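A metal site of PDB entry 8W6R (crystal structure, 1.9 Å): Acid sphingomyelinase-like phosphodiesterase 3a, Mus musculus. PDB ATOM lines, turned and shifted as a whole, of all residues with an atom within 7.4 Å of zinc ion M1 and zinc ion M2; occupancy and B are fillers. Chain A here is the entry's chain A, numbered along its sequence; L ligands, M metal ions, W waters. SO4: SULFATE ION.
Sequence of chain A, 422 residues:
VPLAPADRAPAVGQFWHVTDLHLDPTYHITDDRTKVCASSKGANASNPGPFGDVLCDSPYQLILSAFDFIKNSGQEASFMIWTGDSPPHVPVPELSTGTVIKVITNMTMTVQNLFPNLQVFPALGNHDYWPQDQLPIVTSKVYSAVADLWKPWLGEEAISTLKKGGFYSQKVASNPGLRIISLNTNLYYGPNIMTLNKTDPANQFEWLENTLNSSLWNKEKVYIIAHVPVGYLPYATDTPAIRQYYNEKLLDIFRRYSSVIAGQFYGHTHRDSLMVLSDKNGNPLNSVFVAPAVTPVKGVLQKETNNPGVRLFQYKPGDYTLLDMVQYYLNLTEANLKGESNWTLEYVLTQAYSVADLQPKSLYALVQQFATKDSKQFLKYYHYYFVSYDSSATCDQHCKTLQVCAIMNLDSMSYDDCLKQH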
ATOM      1  N   THR A  19      -9.747   7.298   6.714  1.00  0.00           N
ATOM      2  CA  THR A  19      -8.670   6.630   7.438  1.00  0.00           C
ATOM      3  C   THR A  19      -7.428   6.559   6.560  1.00  0.00           C
ATOM      4  O   THR A  19      -7.506   6.607   5.329  1.00  0.00           O
ATOM      5  CB  THR A  19      -9.082   5.201   7.873  1.00  0.00           C
ATOM      6  OG1 THR A  19      -8.119   4.677   8.789  1.00  0.00           O
ATOM      7  CG2 THR A  19      -9.140   4.262   6.671  1.00  0.00           C
ATOM      8  N   ASP A  20      -6.286   6.437   7.219  1.00  0.00           N
ATOM      9  CA  ASP A  20      -5.008   6.162   6.557  1.00  0.00           C
ATOM     10  C   ASP A  20      -4.742   7.177   5.456  1.00  0.00           C
ATOM     11  O   ASP A  20      -4.550   6.844   4.285  1.00  0.00           O
ATOM     12  CB  ASP A  20      -4.949   4.746   6.024  1.00  0.00           C
ATOM     13  CG  ASP A  20      -4.935   3.729   7.154  1.00  0.00           C
ATOM     14  OD1 ASP A  20      -3.817   3.448   7.645  1.00  0.00           O
ATOM     15  OD2 ASP A  20      -6.031   3.272   7.576  1.00  0.00           O
ATOM     16  N   LEU A  21      -4.740   8.441   5.876  1.00  0.00           N
ATOM     17  CA  LEU A  21      -4.514   9.561   4.976  1.00  0.00           C
ATOM     18  C   LEU A  21      -3.079   9.540   4.457  1.00  0.00           C
ATOM     19  O   LEU A  21      -2.836   9.738   3.254  1.00  0.00           O
ATOM     20  CB  LEU A  21      -4.828  10.851   5.726  1.00  0.00           C
ATOM     21  CG  LEU A  21      -6.297  11.055   6.137  1.00  0.00           C
ATOM     22  CD1 LEU A  21      -6.508  12.417   6.810  1.00  0.00           C
ATOM     23  CD2 LEU A  21      -7.270  10.884   4.991  1.00  0.00           C
ATOM     24  N   HIS A  22      -2.110   9.327   5.348  1.00  0.00           N
ATOM     25  CA  HIS A  22      -0.683   9.217   5.006  1.00  0.00           C
ATOM     26  C   HIS A  22      -0.205  10.318   4.061  1.00  0.00           C
ATOM     27  O   HIS A  22       0.258  10.058   2.939  1.00  0.00           O
ATOM     28  CB  HIS A  22      -0.364   7.860   4.388  1.00  0.00           C
ATOM     29  CG  HIS A  22      -0.460   6.721   5.348  1.00  0.00           C
ATOM     30  ND1 HIS A  22       0.451   6.529   6.365  1.00  0.00           N
ATOM     31  CD2 HIS A  22      -1.313   5.671   5.406  1.00  0.00           C
ATOM     32  CE1 HIS A  22       0.135   5.426   7.032  1.00  0.00           C
ATOM     33  NE2 HIS A  22      -0.920   4.887   6.465  1.00  0.00           N
ATOM     34  N   ASP A  57       2.918   7.684  -1.115  1.00  0.00           N
ATOM     35  CA  ASP A  57       1.850   8.105  -0.235  1.00  0.00           C
ATOM     36  C   ASP A  57       1.166   9.366  -0.808  1.00  0.00           C
ATOM     37  O   ASP A  57       1.508   9.850  -1.879  1.00  0.00           O
ATOM     38  CB  ASP A  57       2.403   8.355   1.160  1.00  0.00           C
ATOM     39  CG  ASP A  57       2.301   7.133   2.039  1.00  0.00           C
ATOM     40  OD1 ASP A  57       1.238   6.489   1.989  1.00  0.00           O
ATOM     41  OD2 ASP A  57       3.280   6.799   2.743  1.00  0.00           O
ATOM     42  N   THR A  83      -9.793   7.208  11.560  1.00  0.00           N
ATOM     43  CA  THR A  83      -9.097   6.183  12.331  1.00  0.00           C
ATOM     44  C   THR A  83      -7.599   6.079  12.051  1.00  0.00           C
ATOM     45  O   THR A  83      -7.057   4.983  11.971  1.00  0.00           O
ATOM     46  CB  THR A  83      -9.797   4.829  12.133  1.00  0.00           C
ATOM     47  OG1 THR A  83      -9.850   4.496  10.736  1.00  0.00           O
ATOM     48  CG2 THR A  83     -11.221   4.879  12.683  1.00  0.00           C
ATOM     49  N   GLY A  84      -6.874   7.203  11.953  1.00  0.00           N
ATOM     50  CA  GLY A  84      -5.437   7.179  12.185  1.00  0.00           C
ATOM     51  C   GLY A  84      -4.570   7.076  10.956  1.00  0.00           C
ATOM     52  O   GLY A  84      -5.034   6.981   9.825  1.00  0.00           O
ATOM     53  N   ASP A  85      -3.252   7.020  11.214  1.00  0.00           N
ATOM     54  CA  ASP A  85      -2.146   7.023  10.248  1.00  0.00           C
ATOM     55  C   ASP A  85      -1.996   8.203   9.310  1.00  0.00           C
ATOM     56  O   ASP A  85      -2.202   8.099   8.100  1.00  0.00           O
ATOM     57  CB  ASP A  85      -2.063   5.780   9.343  1.00  0.00           C
ATOM     58  CG  ASP A  85      -1.528   4.532  10.050  1.00  0.00           C
ATOM     59  OD1 ASP A  85      -0.789   4.713  11.039  1.00  0.00           O
ATOM     60  OD2 ASP A  85      -1.550   3.423   9.445  1.00  0.00           O
ATOM     61  N   SER A  86      -1.486   9.298   9.845  1.00  0.00           N
ATOM     62  CA  SER A  86      -1.382  10.501   9.028  1.00  0.00           C
ATOM     63  C   SER A  86       0.019  10.722   8.462  1.00  0.00           C
ATOM     64  O   SER A  86       0.119  11.252   7.355  1.00  0.00           O
ATOM     65  CB  SER A  86      -1.857  11.703   9.845  1.00  0.00           C
ATOM     66  OG  SER A  86      -3.228  11.541  10.172  1.00  0.00           O
ATOM     67  N   PRO A  87       1.118  10.365   9.144  1.00  0.00           N
ATOM     68  CA  PRO A  87       2.439  10.539   8.536  1.00  0.00           C
ATOM     69  C   PRO A  87       2.689   9.510   7.454  1.00  0.00           C
ATOM     70  O   PRO A  87       2.016   8.459   7.409  1.00  0.00           O
ATOM     71  CB  PRO A  87       3.408  10.338   9.725  1.00  0.00           C
ATOM     72  CG  PRO A  87       2.548  10.646  10.946  1.00  0.00           C
ATOM     73  CD  PRO A  87       1.269   9.963  10.557  1.00  0.00           C
ATOM     74  N   HIS A  89       4.933   6.815   4.810  1.00  0.00           N
ATOM     75  CA  HIS A  89       5.756   5.611   4.967  1.00  0.00           C
ATOM     76  C   HIS A  89       7.167   5.987   4.543  1.00  0.00           C
ATOM     77  O   HIS A  89       7.553   5.811   3.389  1.00  0.00           O
ATOM     78  CB  HIS A  89       5.223   4.474   4.110  1.00  0.00           C
ATOM     79  CG  HIS A  89       3.903   3.955   4.577  1.00  0.00           C
ATOM     80  ND1 HIS A  89       2.707   4.493   4.163  1.00  0.00           N
ATOM     81  CD2 HIS A  89       3.579   2.950   5.427  1.00  0.00           C
ATOM     82  CE1 HIS A  89       1.709   3.837   4.736  1.00  0.00           C
ATOM     83  NE2 HIS A  89       2.214   2.901   5.503  1.00  0.00           N
ATOM     84  N   GLY A 125      -3.198   5.934  14.805  1.00  0.00           N
ATOM     85  CA  GLY A 125      -2.680   4.825  14.037  1.00  0.00           C
ATOM     86  C   GLY A 125      -1.240   4.553  14.437  1.00  0.00           C
ATOM     87  O   GLY A 125      -0.592   5.339  15.124  1.00  0.00           O
ATOM     88  N   ASN A 126      -0.714   3.420  13.958  1.00  0.00           N
ATOM     89  CA  ASN A 126       0.631   3.042  14.380  1.00  0.00           C
ATOM     90  C   ASN A 126       1.677   4.015  13.865  1.00  0.00           C
ATOM     91  O   ASN A 126       2.747   4.136  14.485  1.00  0.00           O
ATOM     92  CB  ASN A 126       0.946   1.596  13.963  1.00  0.00           C
ATOM     93  CG  ASN A 126       0.715   1.361  12.465  1.00  0.00           C
ATOM     94  OD1 ASN A 126      -0.408   1.454  11.989  1.00  0.00           O
ATOM     95  ND2 ASN A 126       1.785   1.031  11.741  1.00  0.00           N
ATOM     96  N   HIS A 127       1.409   4.734  12.764  1.00  0.00           N
ATOM     97  CA  HIS A 127       2.361   5.745  12.312  1.00  0.00           C
ATOM     98  C   HIS A 127       2.205   7.080  13.037  1.00  0.00           C
ATOM     99  O   HIS A 127       3.032   7.982  12.840  1.00  0.00           O
ATOM    100  CB  HIS A 127       2.234   5.966  10.801  1.00  0.00           C
ATOM    101  CG  HIS A 127       2.745   4.825   9.993  1.00  0.00           C
ATOM    102  ND1 HIS A 127       3.997   4.823   9.403  1.00  0.00           N
ATOM    103  CD2 HIS A 127       2.170   3.646   9.666  1.00  0.00           C
ATOM    104  CE1 HIS A 127       4.164   3.682   8.752  1.00  0.00           C
ATOM    105  NE2 HIS A 127       3.072   2.952   8.903  1.00  0.00           N
ATOM    106  N   ASP A 133       4.971   2.758  15.446  1.00  0.00           N
ATOM    107  CA  ASP A 133       4.577   1.512  16.108  1.00  0.00           C
ATOM    108  C   ASP A 133       4.851   1.512  17.610  1.00  0.00           C
ATOM    109  O   ASP A 133       4.268   0.698  18.322  1.00  0.00           O
ATOM    110  CB  ASP A 133       5.256   0.286  15.495  1.00  0.00           C
ATOM    111  CG  ASP A 133       5.084   0.217  13.988  1.00  0.00           C
ATOM    112  OD1 ASP A 133       4.124   0.813  13.456  1.00  0.00           O
ATOM    113  OD2 ASP A 133       5.908  -0.486  13.350  1.00  0.00           O
ATOM    114  N   ASN A 186      -3.075   0.037  18.695  1.00  0.00           N
ATOM    115  CA  ASN A 186      -1.650  -0.059  18.415  1.00  0.00           C
ATOM    116  C   ASN A 186      -0.904  -0.596  19.623  1.00  0.00           C
ATOM    117  O   ASN A 186       0.218  -1.097  19.482  1.00  0.00           O
ATOM    118  CB  ASN A 186      -1.109   1.311  18.028  1.00  0.00           C
ATOM    119  CG  ASN A 186      -1.957   1.983  16.986  1.00  0.00           C
ATOM    120  OD1 ASN A 186      -2.002   1.560  15.829  1.00  0.00           O
ATOM    121  ND2 ASN A 186      -2.680   3.017  17.398  1.00  0.00           N
ATOM    122  N   TYR A 189      -0.507  -4.164  18.740  1.00  0.00           N
ATOM    123  CA  TYR A 189       0.054  -4.460  17.423  1.00  0.00           C
ATOM    124  C   TYR A 189       1.419  -5.117  17.572  1.00  0.00           C
ATOM    125  O   TYR A 189       2.254  -4.650  18.345  1.00  0.00           O
ATOM    126  CB  TYR A 189       0.151  -3.140  16.672  1.00  0.00           C
ATOM    127  CG  TYR A 189       0.617  -3.174  15.245  1.00  0.00           C
ATOM    128  CD1 TYR A 189       0.110  -4.072  14.335  1.00  0.00           C
ATOM    129  CD2 TYR A 189       1.560  -2.244  14.799  1.00  0.00           C
ATOM    130  CE1 TYR A 189       0.555  -4.079  13.015  1.00  0.00           C
ATOM    131  CE2 TYR A 189       1.994  -2.238  13.493  1.00  0.00           C
ATOM    132  CZ  TYR A 189       1.495  -3.144  12.611  1.00  0.00           C
ATOM    133  OH  TYR A 189       1.952  -3.117  11.309  1.00  0.00           O
ATOM    134  N   HIS A 227      -7.695   1.916  15.034  1.00  0.00           N
ATOM    135  CA  HIS A 227      -6.913   1.796  13.808  1.00  0.00           C
ATOM    136  C   HIS A 227      -6.752   0.332  13.399  1.00  0.00           C
ATOM    137  O   HIS A 227      -7.358  -0.135  12.431  1.00  0.00           O
ATOM    138  CB  HIS A 227      -5.548   2.447  13.995  1.00  0.00           C
ATOM    139  CG  HIS A 227      -4.734   2.465  12.745  1.00  0.00           C
ATOM    140  ND1 HIS A 227      -5.151   3.113  11.601  1.00  0.00           N
ATOM    141  CD2 HIS A 227      -3.542   1.905  12.459  1.00  0.00           C
ATOM    142  CE1 HIS A 227      -4.234   2.968  10.663  1.00  0.00           C
ATOM    143  NE2 HIS A 227      -3.247   2.242  11.162  1.00  0.00           N
ATOM    144  N   VAL A 228      -5.921  -0.407  14.138  1.00  0.00           N
ATOM    145  CA  VAL A 228      -5.704  -1.812  13.792  1.00  0.00           C
ATOM    146  C   VAL A 228      -6.928  -2.610  14.196  1.00  0.00           C
ATOM    147  O   VAL A 228      -7.430  -2.440  15.325  1.00  0.00           O
ATOM    148  CB  VAL A 228      -4.446  -2.329  14.473  1.00  0.00           C
ATOM    149  CG1 VAL A 228      -4.163  -3.760  13.983  1.00  0.00           C
ATOM    150  CG2 VAL A 228      -3.307  -1.384  14.195  1.00  0.00           C
ATOM    151  N   GLY A 267      -9.447   0.830  10.430  1.00  0.00           N
ATOM    152  CA  GLY A 267      -8.628   1.067   9.235  1.00  0.00           C
ATOM    153  C   GLY A 267      -7.410   0.143   9.147  1.00  0.00           C
ATOM    154  O   GLY A 267      -7.541  -1.070   9.285  1.00  0.00           O
ATOM    155  N   HIS A 268      -6.243   0.715   8.881  1.00  0.00           N
ATOM    156  CA  HIS A 268      -4.935   0.066   8.936  1.00  0.00           C
ATOM    157  C   HIS A 268      -4.656  -0.882   7.777  1.00  0.00           C
ATOM    158  O   HIS A 268      -3.536  -0.898   7.269  1.00  0.00           O
ATOM    159  CB  HIS A 268      -4.740  -0.703  10.254  1.00  0.00           C
ATOM    160  CG  HIS A 268      -3.459  -1.486  10.312  1.00  0.00           C
ATOM    161  ND1 HIS A 268      -2.219  -0.883  10.492  1.00  0.00           N
ATOM    162  CD2 HIS A 268      -3.220  -2.819  10.201  1.00  0.00           C
ATOM    163  CE1 HIS A 268      -1.281  -1.819  10.480  1.00  0.00           C
ATOM    164  NE2 HIS A 268      -1.867  -2.996  10.305  1.00  0.00           N
ATOM    165  N   THR A 269      -5.610  -1.705   7.374  1.00  0.00           N
ATOM    166  CA  THR A 269      -5.269  -2.649   6.307  1.00  0.00           C
ATOM    167  C   THR A 269      -5.271  -2.023   4.919  1.00  0.00           C
ATOM    168  O   THR A 269      -4.762  -2.656   3.985  1.00  0.00           O
ATOM    169  CB  THR A 269      -6.203  -3.870   6.299  1.00  0.00           C
ATOM    170  OG1 THR A 269      -7.481  -3.501   5.773  1.00  0.00           O
ATOM    171  CG2 THR A 269      -6.355  -4.515   7.695  1.00  0.00           C
ATOM    172  N   HIS A 270      -5.843  -0.818   4.767  1.00  0.00           N
ATOM    173  CA  HIS A 270      -5.916  -0.130   3.477  1.00  0.00           C
ATOM    174  C   HIS A 270      -6.767  -0.910   2.490  1.00  0.00           C
ATOM    175  O   HIS A 270      -6.586  -0.788   1.270  1.00  0.00           O
ATOM    176  CB  HIS A 270      -4.537   0.119   2.862  1.00  0.00           C
ATOM    177  CG  HIS A 270      -3.626   0.967   3.688  1.00  0.00           C
ATOM    178  ND1 HIS A 270      -2.485   1.536   3.165  1.00  0.00           N
ATOM    179  CD2 HIS A 270      -3.673   1.328   4.990  1.00  0.00           C
ATOM    180  CE1 HIS A 270      -1.873   2.238   4.117  1.00  0.00           C
ATOM    181  NE2 HIS A 270      -2.576   2.121   5.227  1.00  0.00           N
ATOM    182  N   ALA A 293      -7.981   2.873   2.547  1.00  0.00           N
ATOM    183  CA  ALA A 293      -7.175   4.061   2.778  1.00  0.00           C
ATOM    184  C   ALA A 293      -7.461   5.140   1.730  1.00  0.00           C
ATOM    185  O   ALA A 293      -7.945   4.856   0.629  1.00  0.00           O
ATOM    186  CB  ALA A 293      -5.687   3.706   2.751  1.00  0.00           C
ATOM    187  N   THR A 295      -4.640   6.859   0.978  1.00  0.00           N
ATOM    188  CA  THR A 295      -3.379   6.648   0.269  1.00  0.00           C
ATOM    189  C   THR A 295      -3.486   5.431  -0.655  1.00  0.00           C
ATOM    190  O   THR A 295      -4.153   4.449  -0.325  1.00  0.00           O
ATOM    191  CB  THR A 295      -2.209   6.465   1.248  1.00  0.00           C
ATOM    192  OG1 THR A 295      -0.983   6.351   0.498  1.00  0.00           O
ATOM    193  CG2 THR A 295      -2.376   5.214   2.085  1.00  0.00           C
ATOM    194  N   VAL A 297      -0.629   3.870  -1.647  1.00  0.00           N
ATOM    195  CA  VAL A 297       0.767   3.433  -1.656  1.00  0.00           C
ATOM    196  C   VAL A 297       0.876   1.913  -1.637  1.00  0.00           C
ATOM    197  O   VAL A 297       0.054   1.208  -1.033  1.00  0.00           O
ATOM    198  CB  VAL A 297       1.489   4.071  -0.462  1.00  0.00           C
ATOM    199  CG1 VAL A 297       1.053   3.418   0.860  1.00  0.00           C
ATOM    200  CG2 VAL A 297       3.020   3.988  -0.612  1.00  0.00           C
HETATM  201  S   SO4 L   1       0.711   0.560   7.692  1.00  0.00           S
HETATM  202  O1  SO4 L   1       0.173   1.749   7.011  1.00  0.00           O
HETATM  203  O2  SO4 L   1       0.441   0.727   9.133  1.00  0.00           O
HETATM  204  O3  SO4 L   1       0.086  -0.642   7.138  1.00  0.00           O
HETATM  205  O4  SO4 L   1       2.180   0.481   7.550  1.00  0.00           O
HETATM  206 ZN    ZN M   1      -1.843   2.985   7.193  1.00  0.00          ZN
HETATM  207 ZN    ZN M   2      -1.439   1.329  10.135  1.00  0.00          ZN
HETATM  208  O   HOH W   1      -2.106   1.096   8.117  1.00  0.00           O
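The backbone NH (N) of Asn 126 is in hydrogen-bond range of the side-chain amide oxygen (OD1) of Asn 186 (2.9 Å). The backbone NH (N) of His 268 sits at hydrogen-bond distance from the side-chain carboxylate (OD2) of Asp 20, at 2.9 Å. ND1 of His 227 is in hydrogen-bond range of O of Thr 83 (2.7 Å). N of His 127 sits at hydrogen-bond distance from OD1 of Asp 85, at 2.8 Å. N of Leu 21 is in hydrogen-bond range of O of Asp 85, 3.4 Å away. The backbone carbonyl oxygen of Asn 126 sits at hydrogen-bond distance from the backbone NH of Asp 133, 2.8 Å away. ND1 of His 22 is in hydrogen-bond range of O of Pro 87. O of His 227 is in hydrogen-bond range of N of Gly 267 (3.0 Å).
The side-chain carboxylate (OD1) of Asp 20 is bound to zinc ion M1 (2.1 Å). Zinc ion M1 is bound by water W1 (2.1 Å). Zinc ion M1 is bound by NE2 of His 22 (2.2 Å). Zinc ion M1 is bound by NE2 of His 270 (2.3 Å). Zinc ion M1 is bound by OD2 of Asp 85. O1 of the ligand is bound to zinc ion M1, 2.4 Å away. Zinc ion M1 has six donor atoms within binding distance.
Of the 26 residues printed, 4 come within 4 Å of zinc ion M1. The nearest printed residue that does not touch zinc ion M1 is His 227 (4.2 Å).
Of the 26 residues printed, 4 come within 4 Å of zinc ion M2. Along chain A the residues within 4 Å of zinc ion M2 span positions 85 to 268. The nearest printed residue that does not touch zinc ion M2 is Asp 20 (4.04 Å).
Zinc ion M2 is bound by OD1 of Asn 126, water W1, OD2 of Asp 85, O2 of the ligand, NE2 of His 227 and ND1 of His 268.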
